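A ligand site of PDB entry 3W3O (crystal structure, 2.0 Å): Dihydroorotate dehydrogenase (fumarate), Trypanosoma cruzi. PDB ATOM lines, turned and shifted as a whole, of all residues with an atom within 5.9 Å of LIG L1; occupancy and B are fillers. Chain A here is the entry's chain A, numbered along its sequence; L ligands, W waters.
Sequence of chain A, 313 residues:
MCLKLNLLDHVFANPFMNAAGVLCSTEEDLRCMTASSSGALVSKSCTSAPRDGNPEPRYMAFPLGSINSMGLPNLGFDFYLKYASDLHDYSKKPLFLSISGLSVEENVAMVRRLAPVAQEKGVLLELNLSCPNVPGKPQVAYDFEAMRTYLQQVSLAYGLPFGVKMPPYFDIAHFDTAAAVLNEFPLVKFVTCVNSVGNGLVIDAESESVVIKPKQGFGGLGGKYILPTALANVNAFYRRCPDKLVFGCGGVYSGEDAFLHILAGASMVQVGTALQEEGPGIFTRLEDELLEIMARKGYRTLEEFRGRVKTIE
The backbone NH (N) of Asn 54 is in hydrogen-bond range of the backbone carbonyl oxygen (O) of Met 70 (2.8 Å). The backbone NH (N) of Met 70 is in hydrogen-bond range of the side-chain amide oxygen (OD1) of Asn 68, at 3.2 Å. The side-chain amide oxygen (OD1) of Asn 128 is in hydrogen-bond range of the backbone NH (N) of Ser 130 (3.0 Å). The side-chain amide nitrogen (ND2) of Asn 195 lies within hydrogen-bond range of the side-chain amide oxygen (OD1) of Asn 128, at 3.5 Å. The backbone carbonyl oxygen (O) of Ser 69 is in hydrogen-bond range of the side-chain amide nitrogen (ND2) of Asn 54, 2.9 Å away. ND2 of Asn 128 is in hydrogen-bond range of OG of Ser 45 (3.5 Å). The backbone carbonyl oxygen (O) of Leu 72 sits at hydrogen-bond distance from the guanidinium group (NE) of Arg 51 (3.2 Å). ND2 of Asn 195 sits at hydrogen-bond distance from OG of Ser 130, 3.1 Å away.
N2 of LIG L1 sits close to N1 of LG2 L2, 3.4 Å away.
Ser 69 touches LIG L1 (OG to C12, 3.6 Å). O of Ser 130 touches O4 of LIG L1 (3.6 Å). Pro 132 touches LIG L1. CD of Lys 215 touches C14 of LIG L1 (3.4 Å). 13 residues have an atom within 4 Å of LIG L1: Lys 44, Asn 54, Asn 68, Ser 69, Met 70, Gly 71, Leu 72, Asn 128, Ser 130, Pro 132, Asn 195, Ser 196 and Lys 215. The nearest printed residue that does not touch LIG L1 is Pro 73 (4.02 Å).
An oxygen (O4) of LIG L1 sits at hydrogen-bond distance from the side-chain amide nitrogen (ND2) of Asn 128 (2.9 Å). The backbone NH (N) of Gly 71 is in hydrogen-bond range of an oxygen (O1) of LIG L1, at 2.9 Å. The side-chain hydroxyl (OG) of Ser 196 lies within hydrogen-bond range of an oxygen (O3) of LIG L1, 2.8 Å away. O2 of LIG L1 is in salt-bridge range of NZ of Lys 44 (3.0 Å). The side-chain hydroxyl (OG) of Ser 45 lies within hydrogen-bond range of a nitrogen (N2) of LG2 L2, 2.8 Å away. ND2 of Asn 68 is in hydrogen-bond range of O3 of LIG L1 (2.9 Å). An oxygen (O1) of LIG L1 sits at hydrogen-bond distance from the backbone NH (N) of Met 70 (3.1 Å). ND2 of Asn 128 is in hydrogen-bond range of O1 of LG2 L2 (3.1 Å). NZ of Lys 44 sits at hydrogen-bond distance from O2 of LG2 L2. N of Leu 72 lies within hydrogen-bond range of O2 of LIG L1, 2.8 Å away. The side-chain amide oxygen (OD1) of Asn 195 sits at hydrogen-bond distance from a nitrogen (N2) of LIG L1, 2.7 Å away. ND2 of Asn 195 lies within hydrogen-bond range of O1 of LG2 L2, at 3.2 Å. An oxygen (O5) of LIG L1 is in hydrogen-bond range of the side-chain amide nitrogen of Asn 54, 3.3 Å away. NZ of Lys 165 sits at hydrogen-bond distance from O3 of LG2 L2, 2.9 Å away.
Water W1 lies within hydrogen-bond range of the side-chain amide oxygen of Asn 68 (3.0 Å) and an oxygen (O1) of LIG L1 (3.0 Å).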
ATOM      1  N   LYS A  44     -18.982 -10.959  33.898  1.00  0.00           N
ATOM      2  CA  LYS A  44     -18.104 -11.417  32.851  1.00  0.00           C
ATOM      3  C   LYS A  44     -17.499 -12.736  33.193  1.00  0.00           C
ATOM      4  O   LYS A  44     -17.012 -12.860  34.287  1.00  0.00           O
ATOM      5  CB  LYS A  44     -16.982 -10.399  32.670  1.00  0.00           C
ATOM      6  CG  LYS A  44     -15.847 -10.764  31.787  1.00  0.00           C
ATOM      7  CD  LYS A  44     -16.205 -10.974  30.332  1.00  0.00           C
ATOM      8  CE  LYS A  44     -15.014 -11.515  29.548  1.00  0.00           C
ATOM      9  NZ  LYS A  44     -15.312 -11.744  28.082  1.00  0.00           N
ATOM     10  N   SER A  45     -17.368 -13.611  32.198  1.00  0.00           N
ATOM     11  CA  SER A  45     -16.784 -14.952  32.376  1.00  0.00           C
ATOM     12  C   SER A  45     -15.376 -14.732  32.916  1.00  0.00           C
ATOM     13  O   SER A  45     -14.656 -13.929  32.391  1.00  0.00           O
ATOM     14  CB  SER A  45     -16.726 -15.714  31.086  1.00  0.00           C
ATOM     15  OG  SER A  45     -18.009 -16.198  30.695  1.00  0.00           O
ATOM     16  N   ARG A  51      -6.935 -11.233  33.468  1.00  0.00           N
ATOM     17  CA  ARG A  51      -6.473 -11.324  32.126  1.00  0.00           C
ATOM     18  C   ARG A  51      -6.731 -10.005  31.362  1.00  0.00           C
ATOM     19  O   ARG A  51      -7.778  -9.375  31.537  1.00  0.00           O
ATOM     20  CB  ARG A  51      -7.186 -12.400  31.351  1.00  0.00           C
ATOM     21  CG  ARG A  51      -6.789 -13.820  31.662  1.00  0.00           C
ATOM     22  CD  ARG A  51      -7.703 -14.777  30.934  1.00  0.00           C
ATOM     23  NE  ARG A  51      -7.679 -14.653  29.455  1.00  0.00           N
ATOM     24  CZ  ARG A  51      -6.880 -15.358  28.658  1.00  0.00           C
ATOM     25  NH1 ARG A  51      -5.963 -16.187  29.168  1.00  0.00           N
ATOM     26  NH2 ARG A  51      -6.949 -15.201  27.345  1.00  0.00           N
ATOM     27  N   ASN A  54      -7.143 -10.132  24.439  1.00  0.00           N
ATOM     28  CA  ASN A  54      -6.456  -9.986  23.175  1.00  0.00           C
ATOM     29  C   ASN A  54      -6.192  -8.543  22.789  1.00  0.00           C
ATOM     30  O   ASN A  54      -6.833  -7.604  23.312  1.00  0.00           O
ATOM     31  CB  ASN A  54      -7.301 -10.652  22.076  1.00  0.00           C
ATOM     32  CG  ASN A  54      -7.283 -12.138  22.128  1.00  0.00           C
ATOM     33  OD1 ASN A  54      -6.369 -12.737  22.723  1.00  0.00           O
ATOM     34  ND2 ASN A  54      -8.290 -12.775  21.514  1.00  0.00           N
ATOM     35  N   ASN A  68     -16.306 -10.452  17.621  1.00  0.00           N
ATOM     36  CA  ASN A  68     -15.429 -10.208  18.755  1.00  0.00           C
ATOM     37  C   ASN A  68     -14.442 -11.356  18.895  1.00  0.00           C
ATOM     38  O   ASN A  68     -14.755 -12.546  18.700  1.00  0.00           O
ATOM     39  CB  ASN A  68     -16.203  -9.995  20.102  1.00  0.00           C
ATOM     40  CG  ASN A  68     -16.473 -11.290  20.824  1.00  0.00           C
ATOM     41  OD1 ASN A  68     -15.592 -11.846  21.516  1.00  0.00           O
ATOM     42  ND2 ASN A  68     -17.673 -11.797  20.702  1.00  0.00           N
ATOM     43  N   SER A  69     -13.247 -10.976  19.278  1.00  0.00           N
ATOM     44  CA  SER A  69     -12.291 -11.932  19.798  1.00  0.00           C
ATOM     45  C   SER A  69     -11.661 -11.321  21.002  1.00  0.00           C
ATOM     46  O   SER A  69     -10.510 -10.961  21.011  1.00  0.00           O
ATOM     47  CB  SER A  69     -11.284 -12.308  18.735  1.00  0.00           C
ATOM     48  OG  SER A  69     -10.427 -13.337  19.253  1.00  0.00           O
ATOM     49  N   MET A  70     -12.469 -11.150  22.050  1.00  0.00           N
ATOM     50  CA  MET A  70     -12.032 -10.424  23.225  1.00  0.00           C
ATOM     51  C   MET A  70     -10.868 -11.134  23.929  1.00  0.00           C
ATOM     52  O   MET A  70      -9.946 -10.506  24.493  1.00  0.00           O
ATOM     53  CB  MET A  70     -13.188 -10.287  24.196  1.00  0.00           C
ATOM     54  CG  MET A  70     -14.429  -9.588  23.678  1.00  0.00           C
ATOM     55  SD  MET A  70     -14.169  -7.933  23.108  1.00  0.00           S
ATOM     56  CE  MET A  70     -13.876  -7.049  24.618  1.00  0.00           C
ATOM     57  N   GLY A  71     -10.897 -12.457  23.945  1.00  0.00           N
ATOM     58  CA  GLY A  71      -9.879 -13.206  24.644  1.00  0.00           C
ATOM     59  C   GLY A  71      -9.999 -13.272  26.172  1.00  0.00           C
ATOM     60  O   GLY A  71      -8.989 -13.278  26.869  1.00  0.00           O
ATOM     61  N   LEU A  72     -11.226 -13.248  26.694  1.00  0.00           N
ATOM     62  CA  LEU A  72     -11.505 -13.383  28.093  1.00  0.00           C
ATOM     63  C   LEU A  72     -10.748 -12.397  28.961  1.00  0.00           C
ATOM     64  O   LEU A  72     -10.246 -12.758  30.002  1.00  0.00           O
ATOM     65  CB  LEU A  72     -11.188 -14.828  28.541  1.00  0.00           C
ATOM     66  CG  LEU A  72     -11.999 -15.613  29.512  1.00  0.00           C
ATOM     67  CD1 LEU A  72     -13.504 -15.447  29.420  1.00  0.00           C
ATOM     68  CD2 LEU A  72     -11.591 -17.093  29.375  1.00  0.00           C
ATOM     69  N   PRO A  73     -10.779 -11.132  28.595  1.00  0.00           N
ATOM     70  CA  PRO A  73     -10.294 -10.106  29.560  1.00  0.00           C
ATOM     71  C   PRO A  73     -11.207 -10.042  30.788  1.00  0.00           C
ATOM     72  O   PRO A  73     -12.421  -9.954  30.634  1.00  0.00           O
ATOM     73  CB  PRO A  73     -10.383  -8.814  28.767  1.00  0.00           C
ATOM     74  CG  PRO A  73     -11.524  -9.007  27.839  1.00  0.00           C
ATOM     75  CD  PRO A  73     -11.534 -10.526  27.480  1.00  0.00           C
ATOM     76  N   SER A 100     -15.263 -19.257  33.338  1.00  0.00           N
ATOM     77  CA  SER A 100     -14.735 -19.800  32.118  1.00  0.00           C
ATOM     78  C   SER A 100     -13.262 -20.183  32.233  1.00  0.00           C
ATOM     79  O   SER A 100     -12.457 -19.691  31.509  1.00  0.00           O
ATOM     80  CB  SER A 100     -15.011 -18.860  30.930  1.00  0.00           C
ATOM     81  OG  SER A 100     -14.482 -19.326  29.736  1.00  0.00           O
ATOM     82  N   LEU A 102      -9.772 -22.166  31.947  1.00  0.00           N
ATOM     83  CA  LEU A 102      -9.091 -22.677  30.772  1.00  0.00           C
ATOM     84  C   LEU A 102      -8.762 -24.195  30.809  1.00  0.00           C
ATOM     85  O   LEU A 102      -8.276 -24.732  29.854  1.00  0.00           O
ATOM     86  CB  LEU A 102      -7.860 -21.830  30.442  1.00  0.00           C
ATOM     87  CG  LEU A 102      -8.118 -20.319  30.250  1.00  0.00           C
ATOM     88  CD1 LEU A 102      -6.961 -19.605  29.609  1.00  0.00           C
ATOM     89  CD2 LEU A 102      -9.361 -20.058  29.480  1.00  0.00           C
ATOM     90  N   ASN A 128     -19.375 -21.557  31.532  1.00  0.00           N
ATOM     91  CA  ASN A 128     -19.204 -21.339  30.129  1.00  0.00           C
ATOM     92  C   ASN A 128     -18.495 -22.505  29.456  1.00  0.00           C
ATOM     93  O   ASN A 128     -17.272 -22.681  29.603  1.00  0.00           O
ATOM     94  CB  ASN A 128     -18.430 -20.036  29.900  1.00  0.00           C
ATOM     95  CG  ASN A 128     -18.301 -19.673  28.430  1.00  0.00           C
ATOM     96  OD1 ASN A 128     -18.756 -20.372  27.593  1.00  0.00           O
ATOM     97  ND2 ASN A 128     -17.708 -18.555  28.149  1.00  0.00           N
ATOM     98  N   SER A 130     -18.512 -22.928  26.100  1.00  0.00           N
ATOM     99  CA  SER A 130     -18.231 -22.470  24.742  1.00  0.00           C
ATOM    100  C   SER A 130     -16.953 -21.779  24.844  1.00  0.00           C
ATOM    101  O   SER A 130     -16.854 -20.611  24.681  1.00  0.00           O
ATOM    102  CB  SER A 130     -19.346 -21.535  24.222  1.00  0.00           C
ATOM    103  OG  SER A 130     -20.479 -21.519  25.088  1.00  0.00           O
ATOM    104  N   CYS A 131     -15.944 -22.548  25.155  1.00  0.00           N
ATOM    105  CA  CYS A 131     -14.723 -22.083  25.671  1.00  0.00           C
ATOM    106  C   CYS A 131     -13.523 -22.950  25.234  1.00  0.00           C
ATOM    107  O   CYS A 131     -13.611 -24.146  25.229  1.00  0.00           O
ATOM    108  CB  CYS A 131     -14.823 -22.131  27.188  1.00  0.00           C
ATOM    109  SG  CYS A 131     -13.286 -21.756  28.016  1.00  0.00           S
ATOM    110  N   PRO A 132     -12.380 -22.339  24.999  1.00  0.00           N
ATOM    111  CA  PRO A 132     -11.171 -23.078  24.675  1.00  0.00           C
ATOM    112  C   PRO A 132     -10.660 -24.093  25.709  1.00  0.00           C
ATOM    113  O   PRO A 132     -10.709 -23.891  26.867  1.00  0.00           O
ATOM    114  CB  PRO A 132     -10.131 -21.969  24.598  1.00  0.00           C
ATOM    115  CG  PRO A 132     -10.912 -20.740  24.291  1.00  0.00           C
ATOM    116  CD  PRO A 132     -12.363 -21.080  24.268  1.00  0.00           C
ATOM    117  N   LYS A 165     -23.525 -22.376  29.779  1.00  0.00           N
ATOM    118  CA  LYS A 165     -23.578 -21.577  28.510  1.00  0.00           C
ATOM    119  C   LYS A 165     -23.037 -22.396  27.351  1.00  0.00           C
ATOM    120  O   LYS A 165     -21.865 -22.864  27.369  1.00  0.00           O
ATOM    121  CB  LYS A 165     -22.767 -20.289  28.662  1.00  0.00           C
ATOM    122  CG  LYS A 165     -22.703 -19.474  27.405  1.00  0.00           C
ATOM    123  CD  LYS A 165     -24.023 -18.720  27.271  1.00  0.00           C
ATOM    124  CE  LYS A 165     -23.849 -17.518  26.341  1.00  0.00           C
ATOM    125  NZ  LYS A 165     -23.126 -16.356  26.868  1.00  0.00           N
ATOM    126  N   ASN A 195     -24.110 -19.094  22.923  1.00  0.00           N
ATOM    127  CA  ASN A 195     -22.901 -18.268  22.767  1.00  0.00           C
ATOM    128  C   ASN A 195     -22.770 -17.769  21.322  1.00  0.00           C
ATOM    129  O   ASN A 195     -23.570 -18.113  20.441  1.00  0.00           O
ATOM    130  CB  ASN A 195     -21.611 -19.041  23.219  1.00  0.00           C
ATOM    131  CG  ASN A 195     -20.567 -18.132  23.871  1.00  0.00           C
ATOM    132  OD1 ASN A 195     -20.151 -17.140  23.287  1.00  0.00           O
ATOM    133  ND2 ASN A 195     -20.209 -18.422  25.142  1.00  0.00           N
ATOM    134  N   SER A 196     -21.763 -16.928  21.082  1.00  0.00           N
ATOM    135  CA  SER A 196     -21.479 -16.398  19.729  1.00  0.00           C
ATOM    136  C   SER A 196     -21.270 -17.494  18.671  1.00  0.00           C
ATOM    137  O   SER A 196     -20.863 -18.610  18.982  1.00  0.00           O
ATOM    138  CB  SER A 196     -20.334 -15.362  19.782  1.00  0.00           C
ATOM    139  OG  SER A 196     -19.181 -16.013  20.214  1.00  0.00           O
ATOM    140  N   PRO A 214      -7.094  -9.732  16.498  1.00  0.00           N
ATOM    141  CA  PRO A 214      -6.695 -11.090  16.823  1.00  0.00           C
ATOM    142  C   PRO A 214      -7.099 -12.134  15.767  1.00  0.00           C
ATOM    143  O   PRO A 214      -8.082 -11.921  15.020  1.00  0.00           O
ATOM    144  CB  PRO A 214      -7.458 -11.383  18.109  1.00  0.00           C
ATOM    145  CG  PRO A 214      -7.778 -10.031  18.666  1.00  0.00           C
ATOM    146  CD  PRO A 214      -8.085  -9.227  17.457  1.00  0.00           C
ATOM    147  N   LYS A 215      -6.361 -13.237  15.691  1.00  0.00           N
ATOM    148  CA  LYS A 215      -6.771 -14.408  14.942  1.00  0.00           C
ATOM    149  C   LYS A 215      -7.086 -14.096  13.465  1.00  0.00           C
ATOM    150  O   LYS A 215      -8.042 -14.627  12.894  1.00  0.00           O
ATOM    151  CB  LYS A 215      -8.027 -15.055  15.585  1.00  0.00           C
ATOM    152  CG  LYS A 215      -7.913 -15.594  17.021  1.00  0.00           C
ATOM    153  CD  LYS A 215      -9.265 -16.272  17.433  1.00  0.00           C
ATOM    154  CE  LYS A 215      -9.901 -17.191  16.335  1.00  0.00           C
ATOM    155  NZ  LYS A 215     -10.966 -18.036  16.877  1.00  0.00           N
ATOM    156  N   GLY A 220     -16.177 -14.444  17.019  1.00  0.00           N
ATOM    157  CA  GLY A 220     -17.523 -14.860  17.242  1.00  0.00           C
ATOM    158  C   GLY A 220     -18.513 -13.806  16.763  1.00  0.00           C
ATOM    159  O   GLY A 220     -18.365 -12.630  17.046  1.00  0.00           O
HETATM  160  O1  LIG L   1     -13.602 -13.542  23.706  1.00  0.00           O
HETATM  161  C1  LIG L   1     -14.323 -13.733  24.741  1.00  0.00           C
HETATM  162  O2  LIG L   1     -13.959 -13.316  25.889  1.00  0.00           O
HETATM  163  C2  LIG L   1     -15.541 -14.462  24.558  1.00  0.00           C
HETATM  164  N1  LIG L   1     -16.340 -14.015  23.448  1.00  0.00           N
HETATM  165  C3  LIG L   1     -17.539 -14.628  23.105  1.00  0.00           C
HETATM  166  O3  LIG L   1     -18.209 -14.253  22.127  1.00  0.00           O
HETATM  167  N2  LIG L   1     -17.932 -15.719  23.874  1.00  0.00           N
HETATM  168  C4  LIG L   1     -17.166 -16.257  24.962  1.00  0.00           C
HETATM  169  O4  LIG L   1     -17.627 -17.237  25.589  1.00  0.00           O
HETATM  170  C5  LIG L   1     -15.928 -15.593  25.295  1.00  0.00           C
HETATM  171  C6  LIG L   1     -15.105 -16.084  26.325  1.00  0.00           C
HETATM  172  C7  LIG L   1     -14.534 -17.528  25.855  1.00  0.00           C
HETATM  173  C8  LIG L   1     -13.218 -17.298  25.217  1.00  0.00           C
HETATM  174  C9  LIG L   1     -13.033 -16.831  23.897  1.00  0.00           C
HETATM  175  C10 LIG L   1     -11.685 -16.650  23.485  1.00  0.00           C
HETATM  176  C11 LIG L   1     -11.496 -16.164  22.225  1.00  0.00           C
HETATM  177  C12 LIG L   1     -10.225 -15.939  21.781  1.00  0.00           C
HETATM  178  C13 LIG L   1      -9.084 -16.206  22.503  1.00  0.00           C
HETATM  179  O5  LIG L   1      -7.855 -15.975  21.941  1.00  0.00           O
HETATM  180  C14 LIG L   1      -7.841 -16.110  20.544  1.00  0.00           C
HETATM  181  C15 LIG L   1      -9.211 -16.688  23.787  1.00  0.00           C
HETATM  182  C16 LIG L   1     -10.532 -16.894  24.226  1.00  0.00           C
HETATM  183  C17 LIG L   1     -10.699 -17.383  25.475  1.00  0.00           C
HETATM  184  C18 LIG L   1     -12.039 -17.541  25.916  1.00  0.00           C
HETATM  185  N1  LG2 L   2     -20.225 -15.239  26.364  1.00  0.00           N
HETATM  186  C1  LG2 L   2     -19.784 -15.790  27.493  1.00  0.00           C
HETATM  187  O1  LG2 L   2     -20.342 -16.850  27.877  1.00  0.00           O
HETATM  188  N2  LG2 L   2     -18.767 -15.267  28.216  1.00  0.00           N
HETATM  189  C2  LG2 L   2     -18.138 -14.120  27.933  1.00  0.00           C
HETATM  190  O2  LG2 L   2     -17.237 -13.644  28.656  1.00  0.00           O
HETATM  191  C3  LG2 L   2     -18.562 -13.453  26.735  1.00  0.00           C
HETATM  192  N3  LG2 L   2     -17.975 -12.351  26.323  1.00  0.00           N
HETATM  193  C4  LG2 L   2     -18.490 -11.605  25.281  1.00  0.00           C
HETATM  194  C5  LG2 L   2     -18.005 -10.333  24.964  1.00  0.00           C
HETATM  195  C6  LG2 L   2     -18.494  -9.649  23.855  1.00  0.00           C
HETATM  196  C7  LG2 L   2     -17.927  -8.319  23.517  1.00  0.00           C
HETATM  197  C8  LG2 L   2     -19.627 -10.189  23.076  1.00  0.00           C
HETATM  198  C9  LG2 L   2     -20.198  -9.498  21.850  1.00  0.00           C
HETATM  199  C10 LG2 L   2     -20.123 -11.412  23.423  1.00  0.00           C
HETATM  200  C11 LG2 L   2     -19.637 -12.119  24.495  1.00  0.00           C
HETATM  201  N4  LG2 L   2     -20.142 -13.391  24.847  1.00  0.00           N
HETATM  202  C12 LG2 L   2     -19.666 -14.053  25.972  1.00  0.00           C
HETATM  203  C13 LG2 L   2     -21.254 -13.956  24.103  1.00  0.00           C
HETATM  204  C14 LG2 L   2     -22.544 -13.257  24.473  1.00  0.00           C
HETATM  205  O3  LG2 L   2     -22.754 -13.626  25.815  1.00  0.00           O
HETATM  206  C15 LG2 L   2     -23.685 -13.860  23.642  1.00  0.00           C
HETATM  207  O4  LG2 L   2     -23.694 -15.241  23.912  1.00  0.00           O
HETATM  208  C16 LG2 L   2     -23.476 -13.613  22.146  1.00  0.00           C
HETATM  209  O5  LG2 L   2     -22.972 -12.272  21.921  1.00  0.00           O
HETATM  210  C17 LG2 L   2     -24.806 -13.734  21.363  1.00  0.00           C
HETATM  211  O6  LG2 L   2     -25.844 -12.822  21.792  1.00  0.00           O
HETATM  212  P1  LG2 L   2     -26.204 -11.469  21.004  1.00  0.00           P
HETATM  213  O7  LG2 L   2     -27.256 -10.740  21.884  1.00  0.00           O
HETATM  214  O8  LG2 L   2     -26.513 -11.966  19.630  1.00  0.00           O
HETATM  215  O9  LG2 L   2     -24.856 -10.782  20.926  1.00  0.00           O
HETATM  216  O   HOH W   1     -14.460 -14.550  20.969  1.00  0.00           O
